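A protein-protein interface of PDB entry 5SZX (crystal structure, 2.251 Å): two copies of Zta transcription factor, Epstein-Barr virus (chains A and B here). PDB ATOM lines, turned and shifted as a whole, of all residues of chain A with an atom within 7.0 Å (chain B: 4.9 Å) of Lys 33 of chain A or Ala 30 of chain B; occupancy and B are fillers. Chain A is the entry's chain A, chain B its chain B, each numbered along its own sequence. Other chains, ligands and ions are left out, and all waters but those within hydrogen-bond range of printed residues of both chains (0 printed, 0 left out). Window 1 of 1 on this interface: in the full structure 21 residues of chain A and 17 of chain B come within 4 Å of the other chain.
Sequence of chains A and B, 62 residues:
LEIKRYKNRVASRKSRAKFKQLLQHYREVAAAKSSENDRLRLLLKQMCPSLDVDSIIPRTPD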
ATOM      1  N   TYR A  26      26.318 -10.614  36.491  1.00  0.00           N
ATOM      2  CA  TYR A  26      27.114  -9.716  35.664  1.00  0.00           C
ATOM      3  C   TYR A  26      27.015 -10.081  34.184  1.00  0.00           C
ATOM      4  O   TYR A  26      27.151  -9.220  33.319  1.00  0.00           O
ATOM      5  CB  TYR A  26      28.575  -9.726  36.122  1.00  0.00           C
ATOM      6  CG  TYR A  26      28.820  -8.995  37.429  1.00  0.00           C
ATOM      7  CD1 TYR A  26      28.030  -7.913  37.804  1.00  0.00           C
ATOM      8  CD2 TYR A  26      29.844  -9.382  38.286  1.00  0.00           C
ATOM      9  CE1 TYR A  26      28.250  -7.241  38.995  1.00  0.00           C
ATOM     10  CE2 TYR A  26      30.072  -8.713  39.484  1.00  0.00           C
ATOM     11  CZ  TYR A  26      29.272  -7.644  39.830  1.00  0.00           C
ATOM     12  OH  TYR A  26      29.490  -6.975  41.015  1.00  0.00           O
ATOM     13  N   ARG A  27      26.764 -11.353  33.893  1.00  0.00           N
ATOM     14  CA  ARG A  27      26.534 -11.780  32.516  1.00  0.00           C
ATOM     15  C   ARG A  27      25.201 -11.256  32.003  1.00  0.00           C
ATOM     16  O   ARG A  27      25.122 -10.711  30.903  1.00  0.00           O
ATOM     17  CB  ARG A  27      26.575 -13.302  32.402  1.00  0.00           C
ATOM     18  CG  ARG A  27      27.975 -13.872  32.336  1.00  0.00           C
ATOM     19  CD  ARG A  27      27.961 -15.386  32.425  1.00  0.00           C
ATOM     20  NE  ARG A  27      27.276 -15.997  31.293  1.00  0.00           N
ATOM     21  CZ  ARG A  27      27.256 -17.305  31.057  1.00  0.00           C
ATOM     22  NH1 ARG A  27      27.881 -18.136  31.882  1.00  0.00           N
ATOM     23  NH2 ARG A  27      26.607 -17.785  30.002  1.00  0.00           N
ATOM     24  N   GLU A  28      24.160 -11.413  32.812  1.00  0.00           N
ATOM     25  CA  GLU A  28      22.824 -10.968  32.432  1.00  0.00           C
ATOM     26  C   GLU A  28      22.778  -9.454  32.261  1.00  0.00           C
ATOM     27  O   GLU A  28      22.089  -8.940  31.384  1.00  0.00           O
ATOM     28  CB  GLU A  28      21.795 -11.410  33.471  1.00  0.00           C
ATOM     29  CG  GLU A  28      21.540 -12.907  33.492  1.00  0.00           C
ATOM     30  CD  GLU A  28      20.674 -13.335  34.661  1.00  0.00           C
ATOM     31  OE1 GLU A  28      20.293 -12.467  35.476  1.00  0.00           O
ATOM     32  OE2 GLU A  28      20.378 -14.543  34.768  1.00  0.00           O
ATOM     33  N   VAL A  29      23.502  -8.740  33.110  1.00  0.00           N
ATOM     34  CA  VAL A  29      23.564  -7.292  32.997  1.00  0.00           C
ATOM     35  C   VAL A  29      24.296  -6.887  31.721  1.00  0.00           C
ATOM     36  O   VAL A  29      23.816  -6.043  30.961  1.00  0.00           O
ATOM     37  CB  VAL A  29      24.248  -6.662  34.219  1.00  0.00           C
ATOM     38  CG1 VAL A  29      24.508  -5.185  33.978  1.00  0.00           C
ATOM     39  CG2 VAL A  29      23.382  -6.852  35.448  1.00  0.00           C
ATOM     40  N   ALA A  30      25.448  -7.506  31.483  1.00  0.00           N
ATOM     41  CA  ALA A  30      26.257  -7.200  30.308  1.00  0.00           C
ATOM     42  C   ALA A  30      25.487  -7.467  29.018  1.00  0.00           C
ATOM     43  O   ALA A  30      25.598  -6.712  28.053  1.00  0.00           O
ATOM     44  CB  ALA A  30      27.546  -8.002  30.329  1.00  0.00           C
ATOM     45  N   ALA A  31      24.708  -8.542  29.006  1.00  0.00           N
ATOM     46  CA  ALA A  31      23.913  -8.884  27.834  1.00  0.00           C
ATOM     47  C   ALA A  31      22.819  -7.851  27.595  1.00  0.00           C
ATOM     48  O   ALA A  31      22.650  -7.358  26.482  1.00  0.00           O
ATOM     49  CB  ALA A  31      23.308 -10.266  27.992  1.00  0.00           C
ATOM     50  N   ALA A  32      22.103  -7.503  28.658  1.00  0.00           N
ATOM     51  CA  ALA A  32      20.973  -6.584  28.565  1.00  0.00           C
ATOM     52  C   ALA A  32      21.389  -5.207  28.061  1.00  0.00           C
ATOM     53  O   ALA A  32      20.730  -4.629  27.199  1.00  0.00           O
ATOM     54  CB  ALA A  32      20.286  -6.460  29.923  1.00  0.00           C
ATOM     55  N   LYS A  33      22.483  -4.686  28.604  1.00  0.00           N
ATOM     56  CA  LYS A  33      22.990  -3.384  28.193  1.00  0.00           C
ATOM     57  C   LYS A  33      23.526  -3.425  26.767  1.00  0.00           C
ATOM     58  O   LYS A  33      23.361  -2.469  26.011  1.00  0.00           O
ATOM     59  CB  LYS A  33      24.059  -2.897  29.169  1.00  0.00           C
ATOM     60  CG  LYS A  33      23.477  -2.473  30.509  1.00  0.00           C
ATOM     61  CD  LYS A  33      24.541  -1.954  31.453  1.00  0.00           C
ATOM     62  CE  LYS A  33      23.917  -1.479  32.756  1.00  0.00           C
ATOM     63  NZ  LYS A  33      24.938  -1.111  33.778  1.00  0.00           N
ATOM     64  N   SER A  34      24.178  -4.526  26.404  1.00  0.00           N
ATOM     65  CA  SER A  34      24.637  -4.708  25.032  1.00  0.00           C
ATOM     66  C   SER A  34      23.440  -4.705  24.090  1.00  0.00           C
ATOM     67  O   SER A  34      23.498  -4.146  22.994  1.00  0.00           O
ATOM     68  CB  SER A  34      25.429  -6.005  24.885  1.00  0.00           C
ATOM     69  OG  SER A  34      26.627  -5.952  25.638  1.00  0.00           O
ATOM     70  N   SER A  35      22.352  -5.325  24.537  1.00  0.00           N
ATOM     71  CA  SER A  35      21.108  -5.337  23.779  1.00  0.00           C
ATOM     72  C   SER A  35      20.547  -3.925  23.668  1.00  0.00           C
ATOM     73  O   SER A  35      20.129  -3.495  22.593  1.00  0.00           O
ATOM     74  CB  SER A  35      20.083  -6.266  24.430  1.00  0.00           C
ATOM     75  OG  SER A  35      18.846  -6.212  23.738  1.00  0.00           O
ATOM     76  N   GLU A  36      20.539  -3.209  24.787  1.00  0.00           N
ATOM     77  CA  GLU A  36      20.084  -1.825  24.800  1.00  0.00           C
ATOM     78  C   GLU A  36      20.952  -0.990  23.869  1.00  0.00           C
ATOM     79  O   GLU A  36      20.441  -0.212  23.063  1.00  0.00           O
ATOM     80  CB  GLU A  36      20.115  -1.246  26.223  1.00  0.00           C
ATOM     81  N   ASN A  37      22.265  -1.184  23.967  1.00  0.00           N
ATOM     82  CA  ASN A  37      23.228  -0.446  23.155  1.00  0.00           C
ATOM     83  C   ASN A  37      22.941  -0.565  21.666  1.00  0.00           C
ATOM     84  O   ASN A  37      22.977   0.424  20.935  1.00  0.00           O
ATOM     85  CB  ASN A  37      24.649  -0.935  23.446  1.00  0.00           C
ATOM     86  CG  ASN A  37      25.691  -0.263  22.569  1.00  0.00           C
ATOM     87  OD1 ASN A  37      26.010  -0.745  21.480  1.00  0.00           O
ATOM     88  ND2 ASN A  37      26.234   0.853  23.043  1.00  0.00           N
ATOM     89  N   ASP A  38      22.645  -1.782  21.227  1.00  0.00           N
ATOM     90  CA  ASP A  38      22.300  -2.031  19.834  1.00  0.00           C
ATOM     91  C   ASP A  38      20.965  -1.398  19.484  1.00  0.00           C
ATOM     92  O   ASP A  38      20.817  -0.783  18.431  1.00  0.00           O
ATOM     93  CB  ASP A  38      22.260  -3.530  19.565  1.00  0.00           C
ATOM     94  CG  ASP A  38      23.596  -4.191  19.803  1.00  0.00           C
ATOM     95  OD1 ASP A  38      24.630  -3.566  19.486  1.00  0.00           O
ATOM     96  OD2 ASP A  38      23.613  -5.320  20.335  1.00  0.00           O
ATOM     97  N   ARG A  39      20.000  -1.535  20.388  1.00  0.00           N
ATOM     98  CA  ARG A  39      18.674  -0.974  20.180  1.00  0.00           C
ATOM     99  C   ARG A  39      18.759   0.541  20.057  1.00  0.00           C
ATOM    100  O   ARG A  39      18.059   1.148  19.246  1.00  0.00           O
ATOM    101  CB  ARG A  39      17.737  -1.367  21.323  1.00  0.00           C
ATOM    102  N   LEU A  40      19.638   1.145  20.851  1.00  0.00           N
ATOM    103  CA  LEU A  40      19.813   2.590  20.818  1.00  0.00           C
ATOM    104  C   LEU A  40      20.510   3.039  19.539  1.00  0.00           C
ATOM    105  O   LEU A  40      20.036   3.943  18.850  1.00  0.00           O
ATOM    106  CB  LEU A  40      20.614   3.054  22.033  1.00  0.00           C
ATOM    107  CG  LEU A  40      19.908   2.967  23.384  1.00  0.00           C
ATOM    108  CD1 LEU A  40      20.888   3.205  24.522  1.00  0.00           C
ATOM    109  CD2 LEU A  40      18.761   3.961  23.443  1.00  0.00           C
ATOM    110  N   TYR B  26      33.152  -9.447  32.611  1.00  0.00           N
ATOM    111  CA  TYR B  26      31.743  -9.096  32.446  1.00  0.00           C
ATOM    112  C   TYR B  26      31.420  -7.791  33.161  1.00  0.00           C
ATOM    113  O   TYR B  26      30.492  -7.077  32.784  1.00  0.00           O
ATOM    114  CB  TYR B  26      30.839 -10.215  32.960  1.00  0.00           C
ATOM    115  CG  TYR B  26      30.819 -11.427  32.059  1.00  0.00           C
ATOM    116  CD1 TYR B  26      30.197 -11.381  30.819  1.00  0.00           C
ATOM    117  CD2 TYR B  26      31.417 -12.617  32.449  1.00  0.00           C
ATOM    118  CE1 TYR B  26      30.176 -12.486  29.990  1.00  0.00           C
ATOM    119  CE2 TYR B  26      31.401 -13.728  31.628  1.00  0.00           C
ATOM    120  CZ  TYR B  26      30.779 -13.657  30.399  1.00  0.00           C
ATOM    121  OH  TYR B  26      30.760 -14.761  29.579  1.00  0.00           O
ATOM    122  N   ARG B  27      32.191  -7.488  34.200  1.00  0.00           N
ATOM    123  CA  ARG B  27      32.060  -6.220  34.901  1.00  0.00           C
ATOM    124  C   ARG B  27      32.532  -5.095  34.000  1.00  0.00           C
ATOM    125  O   ARG B  27      31.849  -4.082  33.844  1.00  0.00           O
ATOM    126  CB  ARG B  27      32.867  -6.231  36.202  1.00  0.00           C
ATOM    127  CG  ARG B  27      32.179  -6.937  37.356  1.00  0.00           C
ATOM    128  CD  ARG B  27      33.109  -7.128  38.548  1.00  0.00           C
ATOM    129  NE  ARG B  27      33.544  -5.867  39.140  1.00  0.00           N
ATOM    130  CZ  ARG B  27      34.231  -5.779  40.275  1.00  0.00           C
ATOM    131  NH1 ARG B  27      34.558  -6.880  40.940  1.00  0.00           N
ATOM    132  NH2 ARG B  27      34.592  -4.591  40.745  1.00  0.00           N
ATOM    133  N   GLU B  28      33.693  -5.287  33.386  1.00  0.00           N
ATOM    134  CA  GLU B  28      34.265  -4.268  32.517  1.00  0.00           C
ATOM    135  C   GLU B  28      33.390  -4.028  31.298  1.00  0.00           C
ATOM    136  O   GLU B  28      33.211  -2.890  30.865  1.00  0.00           O
ATOM    137  CB  GLU B  28      35.671  -4.670  32.083  1.00  0.00           C
ATOM    138  CG  GLU B  28      36.681  -4.631  33.209  1.00  0.00           C
ATOM    139  CD  GLU B  28      38.009  -5.229  32.813  1.00  0.00           C
ATOM    140  OE1 GLU B  28      38.130  -5.705  31.663  1.00  0.00           O
ATOM    141  OE2 GLU B  28      38.935  -5.223  33.652  1.00  0.00           O
ATOM    142  N   VAL B  29      32.825  -5.102  30.762  1.00  0.00           N
ATOM    143  CA  VAL B  29      31.945  -4.989  29.609  1.00  0.00           C
ATOM    144  C   VAL B  29      30.674  -4.233  29.973  1.00  0.00           C
ATOM    145  O   VAL B  29      30.284  -3.293  29.284  1.00  0.00           O
ATOM    146  CB  VAL B  29      31.575  -6.374  29.044  1.00  0.00           C
ATOM    147  CG1 VAL B  29      30.461  -6.253  28.016  1.00  0.00           C
ATOM    148  CG2 VAL B  29      32.799  -7.043  28.437  1.00  0.00           C
ATOM    149  N   ALA B  30      30.047  -4.631  31.075  1.00  0.00           N
ATOM    150  CA  ALA B  30      28.810  -4.002  31.527  1.00  0.00           C
ATOM    151  C   ALA B  30      29.012  -2.521  31.816  1.00  0.00           C
ATOM    152  O   ALA B  30      28.151  -1.697  31.513  1.00  0.00           O
ATOM    153  CB  ALA B  30      28.275  -4.711  32.759  1.00  0.00           C
ATOM    154  N   ALA B  31      30.162  -2.191  32.393  1.00  0.00           N
ATOM    155  CA  ALA B  31      30.476  -0.808  32.727  1.00  0.00           C
ATOM    156  C   ALA B  31      30.631   0.042  31.476  1.00  0.00           C
ATOM    157  O   ALA B  31      30.071   1.135  31.385  1.00  0.00           O
ATOM    158  CB  ALA B  31      31.742  -0.739  33.567  1.00  0.00           C
ATOM    159  N   ALA B  32      31.391  -0.469  30.513  1.00  0.00           N
ATOM    160  CA  ALA B  32      31.662   0.256  29.279  1.00  0.00           C
ATOM    161  C   ALA B  32      30.385   0.510  28.483  1.00  0.00           C
ATOM    162  O   ALA B  32      30.164   1.614  27.983  1.00  0.00           O
ATOM    163  CB  ALA B  32      32.670  -0.507  28.433  1.00  0.00           C
ATOM    164  N   LYS B  33      29.546  -0.515  28.368  1.00  0.00           N
ATOM    165  CA  LYS B  33      28.292  -0.399  27.631  1.00  0.00           C
ATOM    166  C   LYS B  33      27.310   0.539  28.331  1.00  0.00           C
ATOM    167  O   LYS B  33      26.602   1.310  27.679  1.00  0.00           O
ATOM    168  CB  LYS B  33      27.652  -1.778  27.440  1.00  0.00           C
ATOM    169  CG  LYS B  33      28.500  -2.762  26.652  1.00  0.00           C
ATOM    170  CD  LYS B  33      28.708  -2.298  25.224  1.00  0.00           C
ATOM    171  CE  LYS B  33      29.417  -3.358  24.403  1.00  0.00           C
ATOM    172  N   SER B  34      27.277   0.472  29.660  1.00  0.00           N
ATOM    173  CA  SER B  34      26.423   1.352  30.451  1.00  0.00           C
ATOM    174  C   SER B  34      26.771   2.810  30.210  1.00  0.00           C
ATOM    175  O   SER B  34      25.889   3.669  30.147  1.00  0.00           O
ATOM    176  CB  SER B  34      26.547   1.030  31.937  1.00  0.00           C
ATOM    177  OG  SER B  34      25.599   1.766  32.689  1.00  0.00           O
ATOM    178  N   ASN B  37      25.500   3.674  26.748  1.00  0.00           N
ATOM    179  CA  ASN B  37      24.051   3.790  26.829  1.00  0.00           C
ATOM    180  C   ASN B  37      23.616   5.156  27.329  1.00  0.00           C
ATOM    181  O   ASN B  37      22.693   5.760  26.785  1.00  0.00           O
ATOM    182  CB  ASN B  37      23.478   2.698  27.732  1.00  0.00           C
ATOM    183  CG  ASN B  37      23.469   1.341  27.062  1.00  0.00           C
ATOM    184  OD1 ASN B  37      24.157   1.126  26.063  1.00  0.00           O
ATOM    185  ND2 ASN B  37      22.683   0.418  27.604  1.00  0.00           N
ATOM    186  N   THR B  60      17.642  -0.374  31.138  1.00  0.00           N
ATOM    187  CA  THR B  60      18.021  -1.594  31.835  1.00  0.00           C
ATOM    188  C   THR B  60      19.008  -1.374  32.972  1.00  0.00           C
ATOM    189  O   THR B  60      19.981  -0.641  32.813  1.00  0.00           O
ATOM    190  CB  THR B  60      18.640  -2.598  30.853  1.00  0.00           C
ATOM    191  OG1 THR B  60      19.836  -2.038  30.299  1.00  0.00           O
ATOM    192  CG2 THR B  60      17.666  -2.910  29.727  1.00  0.00           C
ATOM    193  N   PRO B  61      18.758  -2.016  34.127  1.00  0.00           N
ATOM    194  CA  PRO B  61      19.670  -1.963  35.273  1.00  0.00           C
ATOM    195  C   PRO B  61      20.984  -2.648  34.888  1.00  0.00           C
ATOM    196  O   PRO B  61      20.966  -3.425  33.930  1.00  0.00           O
ATOM    197  CB  PRO B  61      18.909  -2.733  36.358  1.00  0.00           C
ATOM    198  CG  PRO B  61      18.043  -3.674  35.598  1.00  0.00           C
ATOM    199  CD  PRO B  61      17.600  -2.888  34.394  1.00  0.00           C
ATOM    200  N   ASP B  62      22.091  -2.396  35.584  1.00  0.00           N
ATOM    201  CA  ASP B  62      22.131  -1.619  36.814  1.00  0.00           C
ATOM    202  C   ASP B  62      22.328  -0.125  36.543  1.00  0.00           C
ATOM    203  O   ASP B  62      23.310   0.483  36.979  1.00  0.00           O
ATOM    204  CB  ASP B  62      23.257  -2.143  37.709  1.00  0.00           C
ATOM    205  CG  ASP B  62      22.894  -3.448  38.400  1.00  0.00           C
ATOM    206  OD1 ASP B  62      21.690  -3.690  38.632  1.00  0.00           O
ATOM    207  OD2 ASP B  62      23.817  -4.237  38.702  1.00  0.00           O
ATOM    208  OXT ASP B  62      21.506   0.523  35.893  1.00  0.00           O
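Of the 15 printed residues of chain A, 9 touch a printed residue of chain B.
Of the 13 printed residues of chain B, 9 touch a printed residue of chain A.
The side-chain amino group (NZ) of Lys 33 of chain A is in hydrogen-bond range of the side-chain hydroxyl (OG) of Ser 34 of chain B, at 3.1 Å.
O of Lys 33 of chain A sits at hydrogen-bond distance from ND2 of Asn 37 of chain B.
The side-chain amino group of Lys 33 of chain A lies within salt-bridge range of the chain-end carboxylate of Asp 62 of chain B (3.9 Å).
Lys 33 of chain A touches just these residues of chain B: Ala 30, Ser 34, Asn 37, Thr 60, Pro 61 and Asp 62.
Of the printed residues of chain B, Asn 37 of chain A touches Asn 37 (3.4 Å).
Printed residues of chain A within 4 Å of Tyr 26 of chain B: Tyr 26 (3.8 Å), Arg 27 (3.4 Å) and Ala 30 (3.9 Å).
Of the printed residues of chain B, Val 29 of chain A touches Ala 30 (3.99 Å) and Pro 61 (3.96 Å).
Printed residues of chain B within 4 Å of Ser 34 of chain A: Lys 33 (3.8 Å).
Printed residues of chain B within 4 Å of Ala 30 of chain A: Tyr 26.
The nearest printed residue of chain A that does not touch Ser 34 of chain B is Asn 37 of chain A (6.7 Å).
The backbone carbonyl oxygen (O) of Ala 30 of chain A sits at hydrogen-bond distance from the side-chain hydroxyl (OG) of Ser 34 of chain A (2.7 Å).
The backbone carbonyl oxygen (O) of Lys 33 of chain B sits close to the side-chain amide oxygen (OD1) of Asn 37 of chain B (2.9 Å).
Among the printed residues, pairs that only touch across the chains: Glu 36 of chain A with Asn 37 of chain B (3.4 Å), Asn 37 of chain A with Asn 37 of chain B (3.4 Å), Arg 27 of chain A with Tyr 26 of chain B (3.4 Å), Tyr 26 of chain A with Arg 27 of chain B (3.5 Å), Lys 33 of chain A with Ala 30 of chain B (3.6 Å), Lys 33 of chain A with Thr 60 of chain B (3.7 Å), Lys 33 of chain A with Pro 61 of chain B (3.7 Å), Ser 34 of chain A with Lys 33 of chain B (3.8 Å), Tyr 26 of chain A with Tyr 26 of chain B (3.8 Å), Leu 40 of chain A with Asn 37 of chain B (3.9 Å), Ala 30 of chain A with Tyr 26 of chain B (3.9 Å), Val 29 of chain A with Pro 61 of chain B (3.96 Å) and Val 29 of chain A with Ala 30 of chain B (3.99 Å).
Val 29 of chain A touches Ala 30 of chain B, but with the chains exchanged Ala 30 of chain A does not touch Val 29 of chain B (4.1 Å).
Lys 33 of chain A touches Ala 30 of chain B, but with the chains exchanged Ala 30 of chain A does not touch Lys 33 of chain B (5.1 Å).
Lys 33 of chain A touches Ser 34 of chain B, and with the chains exchanged Ser 34 of chain A touches Lys 33 of chain B.
Asn 37 of chain B touches its own counterpart, Asn 37 of chain A.
Positions printed for both chains: 26, 27, 28, 29, 30, 31, 32, 33, 34 and 37.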
